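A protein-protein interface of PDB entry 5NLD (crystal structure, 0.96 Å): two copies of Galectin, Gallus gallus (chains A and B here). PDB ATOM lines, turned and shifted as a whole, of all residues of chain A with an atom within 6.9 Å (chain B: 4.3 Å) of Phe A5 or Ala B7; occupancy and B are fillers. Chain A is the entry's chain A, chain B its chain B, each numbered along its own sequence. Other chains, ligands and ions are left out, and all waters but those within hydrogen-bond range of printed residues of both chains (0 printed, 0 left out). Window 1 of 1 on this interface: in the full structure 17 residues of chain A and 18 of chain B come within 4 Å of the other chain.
The backbone carbonyl oxygen (O) of Glu A6 sits at hydrogen-bond distance from the backbone NH (N) of Leu B8 (2.8 Å).
The backbone carbonyl oxygen of Glu B6 sits at hydrogen-bond distance from the backbone NH of Leu A8 (2.8 Å).
The backbone carbonyl oxygen of Val A131 sits at hydrogen-bond distance from the backbone NH of Ile B133, at 2.9 Å.
The backbone NH (N) of Ile A122 lies within hydrogen-bond range of the backbone carbonyl oxygen (O) of Phe A5, 2.8 Å away.
The side-chain carboxylate (OE1) of Glu A6 is in hydrogen-bond range of the side-chain amide nitrogen (NE2) of Gln A121, at 3.2 Å.
The backbone carbonyl oxygen (O) of Leu A120 lies within hydrogen-bond range of the backbone NH (N) of Ala A7 (2.8 Å).
N of Ala B7 lies within hydrogen-bond range of O of Leu B120 (2.9 Å).
Leu A3 touches Leu B8 (CD2 to CD2, 3.9 Å).
Phe A5 touches Ala B7 (CZ to CB, 3.9 Å).
CA of Phe A5 touches O of Leu B8 (3.2 Å).
Glu A6 touches Ala B7.
CA of Ala A7 touches O of Glu B6 (3.2 Å).
CA of Phe B5 touches O of Leu A8, at 3.2 Å.
Ile B133 touches Ser A130.
Phe A5 touches just these residues of chain B: Ala B7 and Leu B8.
Ala B7 touches just these residues of chain A: Phe A5 and Glu A6.
Of the printed residues of chain B, Ala A7 touches Glu B6 (3.2 Å).
Printed residues of chain B within 4 Å of Leu A3: Leu B8.
Of the printed residues of chain B, Val A131 touches Ile B133 (2.9 Å).
Of the printed residues of chain A, Glu B6 touches Ala A7 (3.2 Å) and Leu A8 (2.8 Å).
Ile A122 touches none of the printed residues of chain B.
Val A19 touches none of the printed residues of chain B.
The nearest residue of chain B that does not touch Phe A5 is Ile B133 (4.1 Å).
The nearest residue of chain A that does not touch Ala B7 is Ala A7 (4.2 Å).
Of the 18 printed residues of chain A, 7 touch a printed residue of chain B.
Printed residues of chain A that touch a printed residue of chain B: Leu A3, Phe A5, Glu A6, Ala A7, Leu A8, Ser A130 and Val A131.
Of the 9 printed residues of chain B, 5 touch a printed residue of chain A.
Printed residues of chain B that touch a printed residue of chain A: Phe B5, Glu B6, Ala B7, Leu B8 and Ile B133.
Hydrophobic or aromatic side chains of chain B that line the printed part of chain A: Phe B5, Ala B7 and Leu B8.
Along chain B the printed residues that touch a printed residue of chain A span positions 5 to 133.
Phe A5 touches Ala B7, but with the chains exchanged Ala A7 does not touch Phe B5 (4.001 Å).
Phe A5 touches Leu B8, and with the chains exchanged Leu A8 touches Phe B5.
Glu A6 touches Ala B7, and with the chains exchanged Ala A7 touches Glu B6.
Glu A6 touches Leu B8, and with the chains exchanged Leu A8 touches Glu B6.
Of the 10 pairs that touch across the chains among the printed residues, 6 have their exchanged pair printed and touching as well.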
ATOM      1  N   ALA A   2       7.059  34.324 -12.468  1.00  0.00           N
ATOM      2  CA  ALA A   2       5.682  34.606 -12.844  1.00  0.00           C
ATOM      3  C   ALA A   2       4.730  33.614 -12.199  1.00  0.00           C
ATOM      4  O   ALA A   2       5.114  32.514 -11.818  1.00  0.00           O
ATOM      5  CB  ALA A   2       5.527  34.559 -14.366  1.00  0.00           C
ATOM      6  N   LEU A   3       3.465  34.004 -12.123  1.00  0.00           N
ATOM      7  CA  LEU A   3       2.432  33.123 -11.627  1.00  0.00           C
ATOM      8  C   LEU A   3       2.166  32.029 -12.653  1.00  0.00           C
ATOM      9  O   LEU A   3       1.857  32.327 -13.812  1.00  0.00           O
ATOM     10  CB  LEU A   3       1.167  33.933 -11.358  1.00  0.00           C
ATOM     11  CG  LEU A   3      -0.058  33.143 -10.902  1.00  0.00           C
ATOM     12  CD1 LEU A   3       0.135  32.632  -9.522  1.00  0.00           C
ATOM     13  CD2 LEU A   3      -1.308  34.009 -11.021  1.00  0.00           C
ATOM     14  N   ARG A   4       2.267  30.773 -12.216  1.00  0.00           N
ATOM     15  CA  ARG A   4       1.983  29.631 -13.082  1.00  0.00           C
ATOM     16  C   ARG A   4       0.596  29.044 -12.846  1.00  0.00           C
ATOM     17  O   ARG A   4      -0.021  28.538 -13.778  1.00  0.00           O
ATOM     18  CB  ARG A   4       3.043  28.533 -12.925  1.00  0.00           C
ATOM     19  CG  ARG A   4       4.486  29.029 -13.039  1.00  0.00           C
ATOM     20  CD  ARG A   4       4.787  29.776 -14.338  1.00  0.00           C
ATOM     21  NE  ARG A   4       4.917  28.952 -15.538  1.00  0.00           N
ATOM     22  CZ  ARG A   4       6.060  28.442 -15.996  1.00  0.00           C
ATOM     23  NH1 ARG A   4       7.191  28.601 -15.334  1.00  0.00           N
ATOM     24  NH2 ARG A   4       6.076  27.748 -17.127  1.00  0.00           N
ATOM     25  N   PHE A   5       0.098  29.125 -11.616  1.00  0.00           N
ATOM     26  CA  PHE A   5      -1.206  28.550 -11.302  1.00  0.00           C
ATOM     27  C   PHE A   5      -1.703  29.162  -9.999  1.00  0.00           C
ATOM     28  O   PHE A   5      -0.914  29.397  -9.077  1.00  0.00           O
ATOM     29  CB  PHE A   5      -1.075  27.032 -11.110  1.00  0.00           C
ATOM     30  CG  PHE A   5      -2.368  26.330 -10.783  1.00  0.00           C
ATOM     31  CD1 PHE A   5      -3.188  25.841 -11.786  1.00  0.00           C
ATOM     32  CD2 PHE A   5      -2.749  26.135  -9.468  1.00  0.00           C
ATOM     33  CE1 PHE A   5      -4.374  25.197 -11.480  1.00  0.00           C
ATOM     34  CE2 PHE A   5      -3.934  25.490  -9.161  1.00  0.00           C
ATOM     35  CZ  PHE A   5      -4.737  25.021 -10.171  1.00  0.00           C
ATOM     36  N   GLU A   6      -3.009  29.396  -9.915  1.00  0.00           N
ATOM     37  CA  GLU A   6      -3.613  29.786  -8.651  1.00  0.00           C
ATOM     38  C   GLU A   6      -4.982  29.153  -8.556  1.00  0.00           C
ATOM     39  O   GLU A   6      -5.696  29.059  -9.549  1.00  0.00           O
ATOM     40  CB  GLU A   6      -3.717  31.306  -8.527  1.00  0.00           C
ATOM     41  CG  GLU A   6      -4.101  31.777  -7.136  1.00  0.00           C
ATOM     42  CD  GLU A   6      -3.906  33.259  -6.975  1.00  0.00           C
ATOM     43  OE1 GLU A   6      -2.765  33.698  -6.686  1.00  0.00           O
ATOM     44  OE2 GLU A   6      -4.903  33.985  -7.159  1.00  0.00           O
ATOM     45  N   ALA A   7      -5.351  28.698  -7.368  1.00  0.00           N
ATOM     46  CA  ALA A   7      -6.702  28.187  -7.122  1.00  0.00           C
ATOM     47  C   ALA A   7      -7.273  28.854  -5.877  1.00  0.00           C
ATOM     48  O   ALA A   7      -6.549  29.188  -4.931  1.00  0.00           O
ATOM     49  CB  ALA A   7      -6.696  26.689  -6.947  1.00  0.00           C
ATOM     50  N   LEU A   8      -8.591  29.012  -5.898  1.00  0.00           N
ATOM     51  CA  LEU A   8      -9.374  29.646  -4.850  1.00  0.00           C
ATOM     52  C   LEU A   8     -10.541  28.720  -4.498  1.00  0.00           C
ATOM     53  O   LEU A   8     -11.302  28.309  -5.377  1.00  0.00           O
ATOM     54  CB  LEU A   8      -9.917  30.992  -5.357  1.00  0.00           C
ATOM     55  CG  LEU A   8     -11.007  31.678  -4.537  1.00  0.00           C
ATOM     56  CD1 LEU A   8     -10.522  32.008  -3.132  1.00  0.00           C
ATOM     57  CD2 LEU A   8     -11.506  32.926  -5.254  1.00  0.00           C
ATOM     58  N   VAL A  19      -3.090  18.819  -1.754  1.00  0.00           N
ATOM     59  CA  VAL A  19      -2.767  19.414  -3.034  1.00  0.00           C
ATOM     60  C   VAL A  19      -1.648  18.571  -3.627  1.00  0.00           C
ATOM     61  O   VAL A  19      -0.614  18.386  -2.978  1.00  0.00           O
ATOM     62  CB  VAL A  19      -2.315  20.869  -2.870  1.00  0.00           C
ATOM     63  CG1 VAL A  19      -1.894  21.454  -4.218  1.00  0.00           C
ATOM     64  CG2 VAL A  19      -3.423  21.703  -2.209  1.00  0.00           C
ATOM     65  N   VAL A  21       0.805  18.358  -6.917  1.00  0.00           N
ATOM     66  CA  VAL A  21       1.325  19.096  -8.051  1.00  0.00           C
ATOM     67  C   VAL A  21       2.317  18.209  -8.783  1.00  0.00           C
ATOM     68  O   VAL A  21       3.264  17.682  -8.186  1.00  0.00           O
ATOM     69  CB  VAL A  21       2.025  20.384  -7.582  1.00  0.00           C
ATOM     70  CG1 VAL A  21       2.617  21.147  -8.767  1.00  0.00           C
ATOM     71  CG2 VAL A  21       1.049  21.251  -6.799  1.00  0.00           C
ATOM     72  N   LEU A 120      -4.253  28.697  -3.179  1.00  0.00           N
ATOM     73  CA  LEU A 120      -3.045  27.922  -3.492  1.00  0.00           C
ATOM     74  C   LEU A 120      -2.420  28.690  -4.667  1.00  0.00           C
ATOM     75  O   LEU A 120      -3.112  29.005  -5.636  1.00  0.00           O
ATOM     76  CB  LEU A 120      -3.427  26.478  -3.931  1.00  0.00           C
ATOM     77  CG  LEU A 120      -2.346  25.411  -4.082  1.00  0.00           C
ATOM     78  CD1 LEU A 120      -1.656  25.563  -5.408  1.00  0.00           C
ATOM     79  CD2 LEU A 120      -1.354  25.447  -2.936  1.00  0.00           C
ATOM     80  N   GLN A 121      -1.133  28.997  -4.610  1.00  0.00           N
ATOM     81  CA  GLN A 121      -0.463  29.744  -5.666  1.00  0.00           C
ATOM     82  C   GLN A 121       0.867  29.080  -5.987  1.00  0.00           C
ATOM     83  O   GLN A 121       1.579  28.685  -5.073  1.00  0.00           O
ATOM     84  CB  GLN A 121      -0.253  31.116  -5.093  1.00  0.00           C
ATOM     85  CG  GLN A 121       0.467  32.039  -5.959  1.00  0.00           C
ATOM     86  CD  GLN A 121       0.822  33.310  -5.202  1.00  0.00           C
ATOM     87  OE1 GLN A 121       1.729  33.356  -4.353  1.00  0.00           O
ATOM     88  NE2 GLN A 121       0.086  34.357  -5.502  1.00  0.00           N
ATOM     89  N   ILE A 122       1.188  28.956  -7.277  1.00  0.00           N
ATOM     90  CA  ILE A 122       2.417  28.306  -7.713  1.00  0.00           C
ATOM     91  C   ILE A 122       3.142  29.288  -8.627  1.00  0.00           C
ATOM     92  O   ILE A 122       2.559  29.743  -9.614  1.00  0.00           O
ATOM     93  CB  ILE A 122       2.119  26.983  -8.452  1.00  0.00           C
ATOM     94  CG1 ILE A 122       1.224  26.075  -7.594  1.00  0.00           C
ATOM     95  CG2 ILE A 122       3.419  26.293  -8.841  1.00  0.00           C
ATOM     96  CD1 ILE A 122       0.795  24.780  -8.285  1.00  0.00           C
ATOM     97  N   LEU A 123       4.382  29.629  -8.262  1.00  0.00           N
ATOM     98  CA  LEU A 123       5.157  30.655  -8.945  1.00  0.00           C
ATOM     99  C   LEU A 123       6.494  30.117  -9.440  1.00  0.00           C
ATOM    100  O   LEU A 123       7.099  29.214  -8.848  1.00  0.00           O
ATOM    101  CB  LEU A 123       5.477  31.830  -8.004  1.00  0.00           C
ATOM    102  CG  LEU A 123       4.350  32.438  -7.175  1.00  0.00           C
ATOM    103  CD1 LEU A 123       4.909  33.521  -6.279  1.00  0.00           C
ATOM    104  CD2 LEU A 123       3.258  32.991  -8.050  1.00  0.00           C
ATOM    105  N   ILE A 128       3.927  22.971 -15.176  1.00  0.00           N
ATOM    106  CA  ILE A 128       2.938  22.136 -14.524  1.00  0.00           C
ATOM    107  C   ILE A 128       2.307  21.162 -15.513  1.00  0.00           C
ATOM    108  O   ILE A 128       1.914  21.552 -16.612  1.00  0.00           O
ATOM    109  CB  ILE A 128       1.867  23.030 -13.902  1.00  0.00           C
ATOM    110  CG1 ILE A 128       2.492  23.846 -12.767  1.00  0.00           C
ATOM    111  CG2 ILE A 128       0.673  22.208 -13.390  1.00  0.00           C
ATOM    112  CD1 ILE A 128       1.617  24.994 -12.269  1.00  0.00           C
ATOM    113  N   SER A 130      -0.031  18.761 -13.820  1.00  0.00           N
ATOM    114  CA  SER A 130      -1.277  18.470 -13.122  1.00  0.00           C
ATOM    115  C   SER A 130      -1.320  19.186 -11.785  1.00  0.00           C
ATOM    116  O   SER A 130      -0.303  19.282 -11.090  1.00  0.00           O
ATOM    117  CB  SER A 130      -1.414  16.956 -12.883  1.00  0.00           C
ATOM    118  OG  SER A 130      -2.667  16.638 -12.308  1.00  0.00           O
ATOM    119  N   VAL A 131      -2.515  19.645 -11.419  1.00  0.00           N
ATOM    120  CA  VAL A 131      -2.784  20.071 -10.048  1.00  0.00           C
ATOM    121  C   VAL A 131      -4.090  19.403  -9.626  1.00  0.00           C
ATOM    122  O   VAL A 131      -5.101  19.518 -10.319  1.00  0.00           O
ATOM    123  CB  VAL A 131      -2.916  21.592  -9.886  1.00  0.00           C
ATOM    124  CG1 VAL A 131      -3.174  21.947  -8.407  1.00  0.00           C
ATOM    125  CG2 VAL A 131      -1.672  22.312 -10.409  1.00  0.00           C
ATOM    126  N   GLU A 132      -4.055  18.723  -8.485  1.00  0.00           N
ATOM    127  CA  GLU A 132      -5.226  18.077  -7.901  1.00  0.00           C
ATOM    128  C   GLU A 132      -5.409  18.634  -6.501  1.00  0.00           C
ATOM    129  O   GLU A 132      -4.461  18.682  -5.730  1.00  0.00           O
ATOM    130  CB  GLU A 132      -5.032  16.559  -7.822  1.00  0.00           C
ATOM    131  CG  GLU A 132      -6.199  15.810  -7.180  1.00  0.00           C
ATOM    132  CD  GLU A 132      -5.795  14.447  -6.612  1.00  0.00           C
ATOM    133  OE1 GLU A 132      -4.777  13.871  -7.061  1.00  0.00           O
ATOM    134  OE2 GLU A 132      -6.496  13.949  -5.706  1.00  0.00           O
ATOM    135  N   ILE A 133      -6.631  19.059  -6.188  1.00  0.00           N
ATOM    136  CA  ILE A 133      -6.979  19.606  -4.881  1.00  0.00           C
ATOM    137  C   ILE A 133      -8.137  18.768  -4.373  1.00  0.00           C
ATOM    138  O   ILE A 133      -9.191  18.743  -5.003  1.00  0.00           O
ATOM    139  CB  ILE A 133      -7.329  21.099  -4.995  1.00  0.00           C
ATOM    140  CG1 ILE A 133      -6.106  21.861  -5.525  1.00  0.00           C
ATOM    141  CG2 ILE A 133      -7.797  21.658  -3.660  1.00  0.00           C
ATOM    142  CD1 ILE A 133      -6.374  23.307  -5.853  1.00  0.00           C
ATOM    143  N   PHE B   5     -15.292  27.367  -6.459  1.00  0.00           N
ATOM    144  CA  PHE B   5     -13.902  27.073  -6.795  1.00  0.00           C
ATOM    145  C   PHE B   5     -13.536  27.856  -8.043  1.00  0.00           C
ATOM    146  O   PHE B   5     -14.351  27.984  -8.969  1.00  0.00           O
ATOM    147  CB  PHE B   5     -13.737  25.574  -7.082  1.00  0.00           C
ATOM    148  CG  PHE B   5     -12.329  25.153  -7.433  1.00  0.00           C
ATOM    149  CD1 PHE B   5     -11.428  24.788  -6.448  1.00  0.00           C
ATOM    150  CD2 PHE B   5     -11.913  25.115  -8.755  1.00  0.00           C
ATOM    151  CE1 PHE B   5     -10.151  24.395  -6.782  1.00  0.00           C
ATOM    152  CE2 PHE B   5     -10.624  24.733  -9.078  1.00  0.00           C
ATOM    153  CZ  PHE B   5      -9.748  24.369  -8.092  1.00  0.00           C
ATOM    154  N   GLU B   6     -12.304  28.354  -8.088  1.00  0.00           N
ATOM    155  CA  GLU B   6     -11.786  28.957  -9.305  1.00  0.00           C
ATOM    156  C   GLU B   6     -10.316  28.600  -9.441  1.00  0.00           C
ATOM    157  O   GLU B   6      -9.587  28.557  -8.444  1.00  0.00           O
ATOM    158  CB  GLU B   6     -11.966  30.475  -9.275  1.00  0.00           C
ATOM    159  CG  GLU B   6     -11.511  31.185 -10.540  1.00  0.00           C
ATOM    160  CD  GLU B   6     -11.939  32.635 -10.575  1.00  0.00           C
ATOM    161  OE1 GLU B   6     -11.049  33.503 -10.469  1.00  0.00           O
ATOM    162  OE2 GLU B   6     -13.159  32.900 -10.714  1.00  0.00           O
ATOM    163  N   ALA B   7      -9.866  28.335 -10.661  1.00  0.00           N
ATOM    164  CA  ALA B   7      -8.445  28.125 -10.938  1.00  0.00           C
ATOM    165  C   ALA B   7      -8.029  28.970 -12.119  1.00  0.00           C
ATOM    166  O   ALA B   7      -8.825  29.199 -13.035  1.00  0.00           O
ATOM    167  CB  ALA B   7      -8.147  26.678 -11.221  1.00  0.00           C
ATOM    168  N   LEU B   8      -6.778  29.411 -12.083  1.00  0.00           N
ATOM    169  CA  LEU B   8      -6.167  30.241 -13.106  1.00  0.00           C
ATOM    170  C   LEU B   8      -4.851  29.596 -13.527  1.00  0.00           C
ATOM    171  O   LEU B   8      -4.001  29.303 -12.680  1.00  0.00           O
ATOM    172  CB  LEU B   8      -5.904  31.635 -12.543  1.00  0.00           C
ATOM    173  CG  LEU B   8      -5.154  32.616 -13.439  1.00  0.00           C
ATOM    174  CD1 LEU B   8      -5.962  32.946 -14.680  1.00  0.00           C
ATOM    175  CD2 LEU B   8      -4.781  33.877 -12.680  1.00  0.00           C
ATOM    176  N   MET B  13      -5.240  26.755 -20.553  1.00  0.00           N
ATOM    177  CA  MET B  13      -5.638  25.386 -20.202  1.00  0.00           C
ATOM    178  C   MET B  13      -6.533  24.759 -21.275  1.00  0.00           C
ATOM    179  O   MET B  13      -7.344  23.917 -20.965  1.00  0.00           O
ATOM    180  CB  MET B  13      -6.270  25.292 -18.799  1.00  0.00           C
ATOM    181  CG  MET B  13      -7.527  26.125 -18.611  1.00  0.00           C
ATOM    182  SD  MET B  13      -8.483  25.736 -17.114  1.00  0.00           S
ATOM    183  CE  MET B  13      -7.472  26.432 -15.821  1.00  0.00           C
ATOM    184  N   THR B 118      -7.981  30.570 -19.714  1.00  0.00           N
ATOM    185  CA  THR B 118      -7.049  30.446 -18.605  1.00  0.00           C
ATOM    186  C   THR B 118      -7.726  30.221 -17.264  1.00  0.00           C
ATOM    187  O   THR B 118      -7.026  29.984 -16.286  1.00  0.00           O
ATOM    188  CB  THR B 118      -6.164  31.689 -18.505  1.00  0.00           C
ATOM    189  OG1 THR B 118      -7.006  32.829 -18.350  1.00  0.00           O
ATOM    190  CG2 THR B 118      -5.273  31.834 -19.737  1.00  0.00           C
ATOM    191  N   LYS B 119      -9.053  30.275 -17.196  1.00  0.00           N
ATOM    192  CA  LYS B 119      -9.728  30.229 -15.910  1.00  0.00           C
ATOM    193  C   LYS B 119     -10.856  29.211 -15.931  1.00  0.00           C
ATOM    194  O   LYS B 119     -11.599  29.087 -16.921  1.00  0.00           O
ATOM    195  CB  LYS B 119     -10.246  31.632 -15.573  1.00  0.00           C
ATOM    196  CG  LYS B 119     -10.883  31.848 -14.214  1.00  0.00           C
ATOM    197  CD  LYS B 119     -11.248  33.328 -13.993  1.00  0.00           C
ATOM    198  CE  LYS B 119      -9.995  34.229 -13.900  1.00  0.00           C
ATOM    199  NZ  LYS B 119     -10.283  35.697 -13.726  1.00  0.00           N
ATOM    200  N   LEU B 120     -10.969  28.492 -14.819  1.00  0.00           N
ATOM    201  CA  LEU B 120     -12.029  27.532 -14.551  1.00  0.00           C
ATOM    202  C   LEU B 120     -12.787  28.054 -13.332  1.00  0.00           C
ATOM    203  O   LEU B 120     -12.179  28.469 -12.345  1.00  0.00           O
ATOM    204  CB  LEU B 120     -11.406  26.169 -14.224  1.00  0.00           C
ATOM    205  CG  LEU B 120     -12.375  25.099 -13.765  1.00  0.00           C
ATOM    206  CD1 LEU B 120     -13.191  24.575 -14.954  1.00  0.00           C
ATOM    207  CD2 LEU B 120     -11.610  24.011 -13.041  1.00  0.00           C
ATOM    208  N   ILE B 133      -6.856  19.163 -12.548  1.00  0.00           N
ATOM    209  CA  ILE B 133      -6.622  19.845 -13.818  1.00  0.00           C
ATOM    210  C   ILE B 133      -5.309  19.276 -14.354  1.00  0.00           C
ATOM    211  O   ILE B 133      -4.266  19.480 -13.733  1.00  0.00           O
ATOM    212  CB  ILE B 133      -6.560  21.382 -13.599  1.00  0.00           C
ATOM    213  CG1 ILE B 133      -7.884  21.887 -13.005  1.00  0.00           C
ATOM    214  CG2 ILE B 133      -6.231  22.104 -14.903  1.00  0.00           C
ATOM    215  CD1 ILE B 133      -7.826  23.318 -12.506  1.00  0.00           C
